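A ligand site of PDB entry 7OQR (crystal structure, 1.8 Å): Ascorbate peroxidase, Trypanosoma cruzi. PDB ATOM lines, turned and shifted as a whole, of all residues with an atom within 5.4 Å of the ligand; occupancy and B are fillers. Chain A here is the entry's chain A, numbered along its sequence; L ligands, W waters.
A ring nitrogen (NE2) of His 217 binds an iron atom (FE1) of the ligand (2.2 Å).
The backbone NH of His 223 is in hydrogen-bond range of an oxygen (O1) of the ligand (2.9 Å).
An oxygen (O2) of the ligand sits at hydrogen-bond distance from a ring nitrogen (ND1) of His 223, 2.8 Å away.
An oxygen (O1) of the ligand sits at hydrogen-bond distance from the side-chain hydroxyl of Thr 227, 2.9 Å away.
An oxygen (O4) of the ligand sits at hydrogen-bond distance from the backbone NH of Glu 221 (3.0 Å).
ND2 of Asn 226 lies within hydrogen-bond range of O2 of the ligand (3.1 Å).
NH1 of Arg 89 lies within salt-bridge range of O2 of the ligand (3.9 Å).
A ring nitrogen (ND1) of His 223 sits close to the backbone carbonyl oxygen (O) of Glu 221 (3.5 Å).
N of His 223 lies close to O of Tyr 229 (3.1 Å).
The backbone NH of Tyr 229 lies close to the side-chain hydroxyl of Thr 227 (3.5 Å).
The backbone carbonyl oxygen (O) of Ala 189 sits at hydrogen-bond distance from the backbone NH (N) of Ala 277 (3.0 Å).
O of Ala 216 lies within hydrogen-bond range of SG of Cys 219 (3.5 Å).
The backbone carbonyl oxygen (O) of Val 88 is in hydrogen-bond range of the side-chain hydroxyl (OH) of Tyr 309, 3.0 Å away.
The backbone carbonyl oxygen (O) of Lys 124 is in hydrogen-bond range of the guanidinium group (NH1) of Arg 89 (3.1 Å).
The backbone carbonyl oxygen of Tyr 229 sits at hydrogen-bond distance from the backbone NH of Leu 224, 3.2 Å away.
A nitrogen (N3) of the ligand lies close to the indole nitrogen of Trp 92, at 3.3 Å.
Residues that only touch the ligand: Gly 220, Pro 85, Cys 222, Ala 189, Ala 216, Pro 187, Leu 213, Tyr 309, Leu 275, Leu 86, Phe 200, Tyr 229, Val 88, Cys 219 and Ala 277.
22 residues have an atom within 4 Å of the ligand: Pro 85, Leu 86, Val 88, Arg 89, Trp 92, Pro 187, Ala 189, Phe 200, Leu 213, Ala 216, His 217, Cys 219, Gly 220, Glu 221, Cys 222, His 223, Asn 226, Thr 227, Tyr 229, Leu 275, Ala 277 and Tyr 309.
Water W3 lies within hydrogen-bond range of an oxygen (O3) of the ligand (2.6 Å) and the backbone carbonyl oxygen of Ser 82 (3.1 Å).
Water W1 lies within hydrogen-bond range of an oxygen (O4) of the ligand (2.6 Å) and the backbone carbonyl oxygen of Ser 82 (2.8 Å).
Water W2 bridges an oxygen (O2) of the ligand and the guanidinium group of Arg 89.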
ATOM      1  N   SER A  82       7.936  15.412  14.205  1.00  0.00           N
ATOM      2  CA  SER A  82       7.744  14.253  13.292  1.00  0.00           C
ATOM      3  C   SER A  82       7.115  13.085  14.029  1.00  0.00           C
ATOM      4  O   SER A  82       6.529  12.244  13.389  1.00  0.00           O
ATOM      5  CB  SER A  82       8.997  13.817  12.584  1.00  0.00           C
ATOM      6  OG  SER A  82       9.930  13.198  13.442  1.00  0.00           O
ATOM      7  N   PRO A  85       2.609  12.858  13.798  1.00  0.00           N
ATOM      8  CA  PRO A  85       1.963  12.017  12.791  1.00  0.00           C
ATOM      9  C   PRO A  85       2.343  10.532  12.950  1.00  0.00           C
ATOM     10  O   PRO A  85       1.501   9.668  12.755  1.00  0.00           O
ATOM     11  CB  PRO A  85       2.436  12.692  11.478  1.00  0.00           C
ATOM     12  CG  PRO A  85       2.638  14.148  11.862  1.00  0.00           C
ATOM     13  CD  PRO A  85       3.353  13.979  13.203  1.00  0.00           C
ATOM     14  N   LEU A  86       3.548  10.273  13.383  1.00  0.00           N
ATOM     15  CA  LEU A  86       3.993   8.870  13.585  1.00  0.00           C
ATOM     16  C   LEU A  86       3.095   8.188  14.628  1.00  0.00           C
ATOM     17  O   LEU A  86       2.709   7.075  14.419  1.00  0.00           O
ATOM     18  CB  LEU A  86       5.444   8.902  14.071  1.00  0.00           C
ATOM     19  CG  LEU A  86       6.049   7.539  14.374  1.00  0.00           C
ATOM     20  CD1 LEU A  86       6.016   6.630  13.169  1.00  0.00           C
ATOM     21  CD2 LEU A  86       7.460   7.723  14.881  1.00  0.00           C
ATOM     22  N   VAL A  88       0.049   9.011  15.386  1.00  0.00           N
ATOM     23  CA  VAL A  88      -1.320   8.868  14.825  1.00  0.00           C
ATOM     24  C   VAL A  88      -1.369   7.594  13.965  1.00  0.00           C
ATOM     25  O   VAL A  88      -2.322   6.902  14.027  1.00  0.00           O
ATOM     26  CB  VAL A  88      -1.721  10.113  14.032  1.00  0.00           C
ATOM     27  CG1 VAL A  88      -3.004   9.898  13.276  1.00  0.00           C
ATOM     28  CG2 VAL A  88      -1.821  11.328  14.919  1.00  0.00           C
ATOM     29  N   ARG A  89      -0.315   7.347  13.186  1.00  0.00           N
ATOM     30  CA  ARG A  89      -0.256   6.147  12.326  1.00  0.00           C
ATOM     31  C   ARG A  89      -0.139   4.916  13.213  1.00  0.00           C
ATOM     32  O   ARG A  89      -0.765   3.937  12.948  1.00  0.00           O
ATOM     33  CB  ARG A  89       0.963   6.267  11.402  1.00  0.00           C
ATOM     34  CG  ARG A  89       1.123   5.132  10.402  1.00  0.00           C
ATOM     35  CD  ARG A  89       2.334   5.261   9.498  1.00  0.00           C
ATOM     36  NE  ARG A  89       2.555   4.045   8.735  1.00  0.00           N
ATOM     37  CZ  ARG A  89       3.665   3.344   8.692  1.00  0.00           C
ATOM     38  NH1 ARG A  89       4.734   3.740   9.351  1.00  0.00           N
ATOM     39  NH2 ARG A  89       3.720   2.254   7.987  1.00  0.00           N
ATOM     40  N   TRP A  92      -3.496   4.049  14.700  1.00  0.00           N
ATOM     41  CA  TRP A  92      -4.394   3.620  13.596  1.00  0.00           C
ATOM     42  C   TRP A  92      -4.010   2.178  13.174  1.00  0.00           C
ATOM     43  O   TRP A  92      -4.943   1.343  13.085  1.00  0.00           O
ATOM     44  CB  TRP A  92      -4.401   4.661  12.488  1.00  0.00           C
ATOM     45  CG  TRP A  92      -4.325   4.203  11.057  1.00  0.00           C
ATOM     46  CD1 TRP A  92      -3.358   4.558  10.168  1.00  0.00           C
ATOM     47  CD2 TRP A  92      -5.273   3.420  10.317  1.00  0.00           C
ATOM     48  NE1 TRP A  92      -3.594   3.999   8.949  1.00  0.00           N
ATOM     49  CE2 TRP A  92      -4.745   3.256   9.013  1.00  0.00           C
ATOM     50  CE3 TRP A  92      -6.443   2.721  10.644  1.00  0.00           C
ATOM     51  CZ2 TRP A  92      -5.457   2.593   8.004  1.00  0.00           C
ATOM     52  CZ3 TRP A  92      -7.118   2.012   9.665  1.00  0.00           C
ATOM     53  CH2 TRP A  92      -6.614   1.943   8.350  1.00  0.00           C
ATOM     54  N   LYS A 124       5.777  -1.245   8.675  1.00  0.00           N
ATOM     55  CA  LYS A 124       7.233  -0.949   8.658  1.00  0.00           C
ATOM     56  C   LYS A 124       7.442   0.510   9.108  1.00  0.00           C
ATOM     57  O   LYS A 124       6.673   1.420   8.659  1.00  0.00           O
ATOM     58  CB  LYS A 124       7.889  -1.251   7.310  1.00  0.00           C
ATOM     59  CG  LYS A 124       9.415  -1.277   7.370  1.00  0.00           C
ATOM     60  CD  LYS A 124      10.140  -1.586   6.053  1.00  0.00           C
ATOM     61  CE  LYS A 124      11.631  -1.348   6.237  1.00  0.00           C
ATOM     62  NZ  LYS A 124      12.470  -1.773   5.079  1.00  0.00           N
ATOM     63  N   PRO A 187      -4.644  -1.313   4.617  1.00  0.00           N
ATOM     64  CA  PRO A 187      -4.868  -0.962   3.225  1.00  0.00           C
ATOM     65  C   PRO A 187      -3.578  -1.012   2.414  1.00  0.00           C
ATOM     66  O   PRO A 187      -2.485  -0.687   2.856  1.00  0.00           O
ATOM     67  CB  PRO A 187      -5.519   0.409   3.222  1.00  0.00           C
ATOM     68  CG  PRO A 187      -5.596   0.868   4.713  1.00  0.00           C
ATOM     69  CD  PRO A 187      -4.898  -0.199   5.530  1.00  0.00           C
ATOM     70  N   ASP A 188      -3.784  -1.314   1.145  1.00  0.00           N
ATOM     71  CA  ASP A 188      -2.725  -1.352   0.118  1.00  0.00           C
ATOM     72  C   ASP A 188      -2.758  -0.001  -0.620  1.00  0.00           C
ATOM     73  O   ASP A 188      -3.778   0.299  -1.292  1.00  0.00           O
ATOM     74  CB  ASP A 188      -2.963  -2.544  -0.812  1.00  0.00           C
ATOM     75  CG  ASP A 188      -1.927  -2.729  -1.868  1.00  0.00           C
ATOM     76  OD1 ASP A 188      -1.174  -1.749  -2.142  1.00  0.00           O
ATOM     77  OD2 ASP A 188      -1.860  -3.892  -2.389  1.00  0.00           O
ATOM     78  N   ALA A 189      -1.703   0.793  -0.459  1.00  0.00           N
ATOM     79  CA  ALA A 189      -1.608   2.170  -0.999  1.00  0.00           C
ATOM     80  C   ALA A 189      -1.567   2.146  -2.512  1.00  0.00           C
ATOM     81  O   ALA A 189      -1.957   3.185  -3.073  1.00  0.00           O
ATOM     82  CB  ALA A 189      -0.428   2.903  -0.496  1.00  0.00           C
ATOM     83  N   VAL A 196     -10.114   0.167  -1.080  1.00  0.00           N
ATOM     84  CA  VAL A 196     -10.281   1.070   0.103  1.00  0.00           C
ATOM     85  C   VAL A 196     -11.630   0.772   0.764  1.00  0.00           C
ATOM     86  O   VAL A 196     -11.653   0.543   1.917  1.00  0.00           O
ATOM     87  CB  VAL A 196     -10.169   2.538  -0.328  1.00  0.00           C
ATOM     88  CG1 VAL A 196     -10.645   3.465   0.765  1.00  0.00           C
ATOM     89  CG2 VAL A 196      -8.759   2.893  -0.756  1.00  0.00           C
ATOM     90  N   PHE A 200     -12.221  -0.606   4.654  1.00  0.00           N
ATOM     91  CA  PHE A 200     -12.941   0.236   5.642  1.00  0.00           C
ATOM     92  C   PHE A 200     -14.325  -0.343   5.963  1.00  0.00           C
ATOM     93  O   PHE A 200     -14.720  -0.266   7.159  1.00  0.00           O
ATOM     94  CB  PHE A 200     -12.943   1.708   5.244  1.00  0.00           C
ATOM     95  CG  PHE A 200     -11.618   2.378   5.532  1.00  0.00           C
ATOM     96  CD1 PHE A 200     -10.582   2.277   4.618  1.00  0.00           C
ATOM     97  CD2 PHE A 200     -11.385   3.042   6.744  1.00  0.00           C
ATOM     98  CE1 PHE A 200      -9.364   2.883   4.903  1.00  0.00           C
ATOM     99  CE2 PHE A 200     -10.169   3.634   7.018  1.00  0.00           C
ATOM    100  CZ  PHE A 200      -9.161   3.527   6.108  1.00  0.00           C
ATOM    101  N   LEU A 213     -11.279   9.688   8.016  1.00  0.00           N
ATOM    102  CA  LEU A 213     -10.053   8.996   8.530  1.00  0.00           C
ATOM    103  C   LEU A 213      -8.912   9.186   7.538  1.00  0.00           C
ATOM    104  O   LEU A 213      -7.807   9.559   7.971  1.00  0.00           O
ATOM    105  CB  LEU A 213     -10.333   7.536   8.843  1.00  0.00           C
ATOM    106  CG  LEU A 213     -11.252   7.249  10.021  1.00  0.00           C
ATOM    107  CD1 LEU A 213     -11.630   5.778  10.010  1.00  0.00           C
ATOM    108  CD2 LEU A 213     -10.607   7.658  11.313  1.00  0.00           C
ATOM    109  N   ILE A 214      -9.151   9.027   6.211  1.00  0.00           N
ATOM    110  CA  ILE A 214      -8.052   9.158   5.219  1.00  0.00           C
ATOM    111  C   ILE A 214      -7.549  10.600   5.192  1.00  0.00           C
ATOM    112  O   ILE A 214      -6.344  10.791   5.010  1.00  0.00           O
ATOM    113  CB  ILE A 214      -8.530   8.641   3.834  1.00  0.00           C
ATOM    114  CG1 ILE A 214      -8.735   7.134   3.867  1.00  0.00           C
ATOM    115  CG2 ILE A 214      -7.515   9.032   2.765  1.00  0.00           C
ATOM    116  CD1 ILE A 214      -9.393   6.608   2.604  1.00  0.00           C
ATOM    117  N   ALA A 216      -6.489  12.145   7.639  1.00  0.00           N
ATOM    118  CA  ALA A 216      -5.317  12.210   8.565  1.00  0.00           C
ATOM    119  C   ALA A 216      -4.020  12.477   7.804  1.00  0.00           C
ATOM    120  O   ALA A 216      -3.084  13.009   8.380  1.00  0.00           O
ATOM    121  CB  ALA A 216      -5.222  10.979   9.445  1.00  0.00           C
ATOM    122  N   HIS A 217      -3.952  12.206   6.500  1.00  0.00           N
ATOM    123  CA  HIS A 217      -2.747  12.471   5.675  1.00  0.00           C
ATOM    124  C   HIS A 217      -2.534  13.978   5.497  1.00  0.00           C
ATOM    125  O   HIS A 217      -1.518  14.303   5.010  1.00  0.00           O
ATOM    126  CB  HIS A 217      -2.905  11.772   4.330  1.00  0.00           C
ATOM    127  CG  HIS A 217      -2.706  10.315   4.424  1.00  0.00           C
ATOM    128  ND1 HIS A 217      -2.862   9.518   3.281  1.00  0.00           N
ATOM    129  CD2 HIS A 217      -2.265   9.512   5.409  1.00  0.00           C
ATOM    130  CE1 HIS A 217      -2.565   8.264   3.606  1.00  0.00           C
ATOM    131  NE2 HIS A 217      -2.233   8.227   4.926  1.00  0.00           N
ATOM    132  N   CYS A 219      -1.469  15.496   7.811  1.00  0.00           N
ATOM    133  CA  CYS A 219      -0.214  15.585   8.598  1.00  0.00           C
ATOM    134  C   CYS A 219       0.728  14.438   8.278  1.00  0.00           C
ATOM    135  O   CYS A 219       0.270  13.371   7.912  1.00  0.00           O
ATOM    136  CB  CYS A 219      -0.517  15.685  10.091  1.00  0.00           C
ATOM    137  SG  CYS A 219      -0.981  14.161  10.960  1.00  0.00           S
ATOM    138  N   GLY A 220       2.026  14.675   8.430  1.00  0.00           N
ATOM    139  CA  GLY A 220       3.034  13.621   8.240  1.00  0.00           C
ATOM    140  C   GLY A 220       3.512  13.500   6.802  1.00  0.00           C
ATOM    141  O   GLY A 220       3.188  14.349   6.007  1.00  0.00           O
ATOM    142  N   GLU A 221       4.256  12.434   6.526  1.00  0.00           N
ATOM    143  CA  GLU A 221       4.829  12.220   5.187  1.00  0.00           C
ATOM    144  C   GLU A 221       5.229  10.757   5.005  1.00  0.00           C
ATOM    145  O   GLU A 221       5.237  10.025   5.963  1.00  0.00           O
ATOM    146  CB  GLU A 221       6.042  13.126   5.001  1.00  0.00           C
ATOM    147  CG  GLU A 221       7.229  12.744   5.856  1.00  0.00           C
ATOM    148  CD  GLU A 221       8.236  13.867   6.020  1.00  0.00           C
ATOM    149  OE1 GLU A 221       8.005  14.737   6.802  1.00  0.00           O
ATOM    150  OE2 GLU A 221       9.210  13.865   5.358  1.00  0.00           O
ATOM    151  N   CYS A 222       5.506  10.390   3.768  1.00  0.00           N
ATOM    152  CA  CYS A 222       5.962   9.028   3.413  1.00  0.00           C
ATOM    153  C   CYS A 222       7.497   9.013   3.417  1.00  0.00           C
ATOM    154  O   CYS A 222       8.122   9.988   3.089  1.00  0.00           O
ATOM    155  CB  CYS A 222       5.399   8.581   2.073  1.00  0.00           C
ATOM    156  SG  CYS A 222       3.590   8.570   2.027  1.00  0.00           S
ATOM    157  N   HIS A 223       8.035   7.879   3.796  1.00  0.00           N
ATOM    158  CA  HIS A 223       9.485   7.677   3.908  1.00  0.00           C
ATOM    159  C   HIS A 223       9.857   6.484   3.050  1.00  0.00           C
ATOM    160  O   HIS A 223       9.275   5.366   3.263  1.00  0.00           O
ATOM    161  CB  HIS A 223       9.887   7.456   5.360  1.00  0.00           C
ATOM    162  CG  HIS A 223       9.384   8.454   6.346  1.00  0.00           C
ATOM    163  ND1 HIS A 223       8.140   8.328   6.926  1.00  0.00           N
ATOM    164  CD2 HIS A 223       9.914   9.611   6.835  1.00  0.00           C
ATOM    165  CE1 HIS A 223       7.907   9.368   7.700  1.00  0.00           C
ATOM    166  NE2 HIS A 223       8.971  10.166   7.701  1.00  0.00           N
ATOM    167  N   LEU A 224      10.854   6.668   2.200  1.00  0.00           N
ATOM    168  CA  LEU A 224      11.244   5.619   1.244  1.00  0.00           C
ATOM    169  C   LEU A 224      11.637   4.364   2.034  1.00  0.00           C
ATOM    170  O   LEU A 224      11.279   3.230   1.606  1.00  0.00           O
ATOM    171  CB  LEU A 224      12.409   6.164   0.439  1.00  0.00           C
ATOM    172  CG  LEU A 224      12.743   5.410  -0.841  1.00  0.00           C
ATOM    173  CD1 LEU A 224      11.655   5.641  -1.899  1.00  0.00           C
ATOM    174  CD2 LEU A 224      14.127   5.841  -1.393  1.00  0.00           C
ATOM    175  N   ASN A 226      10.491   3.216   4.856  1.00  0.00           N
ATOM    176  CA  ASN A 226       9.359   2.507   5.487  1.00  0.00           C
ATOM    177  C   ASN A 226       8.473   1.807   4.467  1.00  0.00           C
ATOM    178  O   ASN A 226       8.155   0.634   4.616  1.00  0.00           O
ATOM    179  CB  ASN A 226       8.515   3.431   6.367  1.00  0.00           C
ATOM    180  CG  ASN A 226       9.313   3.990   7.532  1.00  0.00           C
ATOM    181  OD1 ASN A 226      10.342   3.428   7.900  1.00  0.00           O
ATOM    182  ND2 ASN A 226       8.705   4.975   8.186  1.00  0.00           N
ATOM    183  N   THR A 227       7.996   2.544   3.461  1.00  0.00           N
ATOM    184  CA  THR A 227       6.945   2.034   2.557  1.00  0.00           C
ATOM    185  C   THR A 227       7.318   2.187   1.076  1.00  0.00           C
ATOM    186  O   THR A 227       6.447   1.836   0.282  1.00  0.00           O
ATOM    187  CB  THR A 227       5.642   2.805   2.731  1.00  0.00           C
ATOM    188  OG1 THR A 227       5.909   4.153   2.460  1.00  0.00           O
ATOM    189  CG2 THR A 227       5.023   2.548   4.085  1.00  0.00           C
ATOM    190  N   TYR A 229       7.421   4.933  -0.549  1.00  0.00           N
ATOM    191  CA  TYR A 229       6.717   6.168  -0.968  1.00  0.00           C
ATOM    192  C   TYR A 229       7.475   7.343  -0.327  1.00  0.00           C
ATOM    193  O   TYR A 229       8.084   7.088   0.748  1.00  0.00           O
ATOM    194  CB  TYR A 229       5.269   6.116  -0.513  1.00  0.00           C
ATOM    195  CG  TYR A 229       4.436   5.093  -1.230  1.00  0.00           C
ATOM    196  CD1 TYR A 229       4.214   5.152  -2.599  1.00  0.00           C
ATOM    197  CD2 TYR A 229       3.971   3.986  -0.566  1.00  0.00           C
ATOM    198  CE1 TYR A 229       3.392   4.237  -3.250  1.00  0.00           C
ATOM    199  CE2 TYR A 229       3.148   3.067  -1.200  1.00  0.00           C
ATOM    200  CZ  TYR A 229       2.881   3.163  -2.544  1.00  0.00           C
ATOM    201  OH  TYR A 229       2.085   2.173  -3.070  1.00  0.00           O
ATOM    202  N   PHE A 233       1.920  15.128   2.031  1.00  0.00           N
ATOM    203  CA  PHE A 233       0.649  15.278   1.308  1.00  0.00           C
ATOM    204  C   PHE A 233       0.296  16.761   1.270  1.00  0.00           C
ATOM    205  O   PHE A 233      -0.416  17.125   0.400  1.00  0.00           O
ATOM    206  CB  PHE A 233      -0.421  14.426   1.951  1.00  0.00           C
ATOM    207  CG  PHE A 233      -0.001  12.987   2.160  1.00  0.00           C
ATOM    208  CD1 PHE A 233       0.649  12.599   3.296  1.00  0.00           C
ATOM    209  CD2 PHE A 233      -0.352  12.054   1.199  1.00  0.00           C
ATOM    210  CE1 PHE A 233       0.968  11.266   3.499  1.00  0.00           C
ATOM    211  CE2 PHE A 233      -0.083  10.719   1.412  1.00  0.00           C
ATOM    212  CZ  PHE A 233       0.632  10.341   2.536  1.00  0.00           C
ATOM    213  N   LEU A 275      -0.781   9.068  -2.904  1.00  0.00           N
ATOM    214  CA  LEU A 275      -0.753   7.639  -3.229  1.00  0.00           C
ATOM    215  C   LEU A 275      -1.871   7.347  -4.202  1.00  0.00           C
ATOM    216  O   LEU A 275      -2.904   8.037  -4.195  1.00  0.00           O
ATOM    217  CB  LEU A 275      -0.910   6.857  -1.932  1.00  0.00           C
ATOM    218  CG  LEU A 275       0.153   7.101  -0.872  1.00  0.00           C
ATOM    219  CD1 LEU A 275      -0.370   6.746   0.508  1.00  0.00           C
ATOM    220  CD2 LEU A 275       1.418   6.362  -1.146  1.00  0.00           C
ATOM    221  N   ALA A 277      -4.124   5.189  -3.726  1.00  0.00           N
ATOM    222  CA  ALA A 277      -5.353   5.029  -2.915  1.00  0.00           C
ATOM    223  C   ALA A 277      -5.949   6.406  -2.561  1.00  0.00           C
ATOM    224  O   ALA A 277      -7.170   6.503  -2.506  1.00  0.00           O
ATOM    225  CB  ALA A 277      -5.038   4.270  -1.671  1.00  0.00           C
ATOM    226  N   PHE A 305     -13.866  13.668  11.715  1.00  0.00           N
ATOM    227  CA  PHE A 305     -12.614  12.933  12.034  1.00  0.00           C
ATOM    228  C   PHE A 305     -12.588  12.526  13.505  1.00  0.00           C
ATOM    229  O   PHE A 305     -12.300  11.379  13.800  1.00  0.00           O
ATOM    230  CB  PHE A 305     -11.382  13.735  11.690  1.00  0.00           C
ATOM    231  CG  PHE A 305     -10.149  12.950  11.982  1.00  0.00           C
ATOM    232  CD1 PHE A 305      -9.520  12.962  13.238  1.00  0.00           C
ATOM    233  CD2 PHE A 305      -9.577  12.186  10.985  1.00  0.00           C
ATOM    234  CE1 PHE A 305      -8.424  12.161  13.472  1.00  0.00           C
ATOM    235  CE2 PHE A 305      -8.449  11.415  11.223  1.00  0.00           C
ATOM    236  CZ  PHE A 305      -7.881  11.391  12.478  1.00  0.00           C
ATOM    237  N   TYR A 309     -12.296   8.687  14.551  1.00  0.00           N
ATOM    238  CA  TYR A 309     -10.997   8.267  15.130  1.00  0.00           C
ATOM    239  C   TYR A 309     -11.237   7.776  16.550  1.00  0.00           C
ATOM    240  O   TYR A 309     -10.628   6.762  16.929  1.00  0.00           O
ATOM    241  CB  TYR A 309      -9.980   9.398  15.087  1.00  0.00           C
ATOM    242  CG  TYR A 309      -8.553   8.945  15.268  1.00  0.00           C
ATOM    243  CD1 TYR A 309      -7.876   8.286  14.237  1.00  0.00           C
ATOM    244  CD2 TYR A 309      -7.843   9.215  16.405  1.00  0.00           C
ATOM    245  CE1 TYR A 309      -6.570   7.830  14.400  1.00  0.00           C
ATOM    246  CE2 TYR A 309      -6.506   8.849  16.557  1.00  0.00           C
ATOM    247  CZ  TYR A 309      -5.849   8.144  15.543  1.00  0.00           C
ATOM    248  OH  TYR A 309      -4.546   7.784  15.762  1.00  0.00           O
ATOM    249  N   LEU A 312     -12.468   4.355  15.948  1.00  0.00           N
ATOM    250  CA  LEU A 312     -11.329   3.490  15.527  1.00  0.00           C
ATOM    251  C   LEU A 312     -10.545   2.982  16.756  1.00  0.00           C
ATOM    252  O   LEU A 312     -10.157   1.812  16.785  1.00  0.00           O
ATOM    253  CB  LEU A 312     -10.446   4.308  14.586  1.00  0.00           C
ATOM    254  CG  LEU A 312      -9.161   3.606  14.101  1.00  0.00           C
ATOM    255  CD1 LEU A 312      -9.467   2.446  13.207  1.00  0.00           C
ATOM    256  CD2 LEU A 312      -8.269   4.578  13.352  1.00  0.00           C
HETATM  257  C1  LIG L   1       1.405   7.745   6.397  1.00  0.00           C
HETATM  258  C2  LIG L   1      -1.029   4.685   3.474  1.00  0.00           C
HETATM  259  C3  LIG L   1      -5.056   5.592   5.849  1.00  0.00           C
HETATM  260  C4  LIG L   1      -2.503   8.269   8.931  1.00  0.00           C
HETATM  261  C5  LIG L   1       1.081   6.796   5.427  1.00  0.00           C
HETATM  262  C6  LIG L   1       2.046   6.186   4.595  1.00  0.00           C
HETATM  263  C7  LIG L   1       1.379   5.366   3.724  1.00  0.00           C
HETATM  264  C8  LIG L   1       0.051   5.366   4.126  1.00  0.00           C
HETATM  265  C9  LIG L   1       1.819   4.431   2.628  1.00  0.00           C
HETATM  266  C10 LIG L   1       3.480   6.478   4.588  1.00  0.00           C
HETATM  267  C11 LIG L   1       4.104   5.734   5.794  1.00  0.00           C
HETATM  268  C12 LIG L   1       5.664   5.880   5.807  1.00  0.00           C
HETATM  269  O1  LIG L   1       6.412   5.739   4.811  1.00  0.00           O
HETATM  270  O2  LIG L   1       6.283   6.285   6.815  1.00  0.00           O
HETATM  271  C13 LIG L   1      -2.363   4.688   3.852  1.00  0.00           C
HETATM  272  C14 LIG L   1      -3.455   4.085   3.088  1.00  0.00           C
HETATM  273  C15 LIG L   1      -4.577   4.480   3.725  1.00  0.00           C
HETATM  274  C16 LIG L   1      -4.170   5.230   4.877  1.00  0.00           C
HETATM  275  C17 LIG L   1      -3.252   3.298   1.795  1.00  0.00           C
HETATM  276  C18 LIG L   1      -6.002   4.117   3.426  1.00  0.00           C
HETATM  277  C19 LIG L   1      -6.263   4.151   2.120  1.00  0.00           C
HETATM  278  C20 LIG L   1      -4.775   6.238   6.998  1.00  0.00           C
HETATM  279  C21 LIG L   1      -5.538   6.446   8.113  1.00  0.00           C
HETATM  280  C22 LIG L   1      -4.815   7.260   8.984  1.00  0.00           C
HETATM  281  C23 LIG L   1      -3.489   7.431   8.437  1.00  0.00           C
HETATM  282  C24 LIG L   1      -6.845   5.913   8.324  1.00  0.00           C
HETATM  283  C25 LIG L   1      -5.274   7.673  10.376  1.00  0.00           C
HETATM  284  C26 LIG L   1      -6.530   7.804  10.804  1.00  0.00           C
HETATM  285  C27 LIG L   1      -1.229   8.357   8.461  1.00  0.00           C
HETATM  286  C28 LIG L   1      -0.280   9.326   9.066  1.00  0.00           C
HETATM  287  C29 LIG L   1       0.800   9.181   8.280  1.00  0.00           C
HETATM  288  C30 LIG L   1       0.435   8.176   7.264  1.00  0.00           C
HETATM  289  C31 LIG L   1      -0.528  10.266  10.237  1.00  0.00           C
HETATM  290  C32 LIG L   1       2.146   9.830   8.402  1.00  0.00           C
HETATM  291  C33 LIG L   1       3.148   9.071   9.278  1.00  0.00           C
HETATM  292  C34 LIG L   1       4.380   9.873   9.574  1.00  0.00           C
HETATM  293  O3  LIG L   1       5.301   9.189  10.133  1.00  0.00           O
HETATM  294  O4  LIG L   1       4.592  11.093   9.170  1.00  0.00           O
HETATM  295  N1  LIG L   1      -0.125   6.297   5.118  1.00  0.00           N
HETATM  296  N2  LIG L   1      -2.895   5.365   4.887  1.00  0.00           N
HETATM  297  N3  LIG L   1      -3.534   6.799   7.253  1.00  0.00           N
HETATM  298  N4  LIG L   1      -0.818   7.682   7.421  1.00  0.00           N
HETATM  299 FE1  LIG L   1      -1.808   6.546   6.201  1.00  0.00          FE
HETATM  300  O   HOH W   1       5.806  12.857  10.713  1.00  0.00           O
HETATM  301  O   HOH W   2       5.489   6.481   9.409  1.00  0.00           O
HETATM  302  O   HOH W   3       7.367  10.373  11.122  1.00  0.00           O
HETATM  303  O   HOH W   4      -0.952   4.516   7.453  1.00  0.00           O
HETATM  304  O   HOH W   5      -2.622   2.388   6.147  1.00  0.00           O
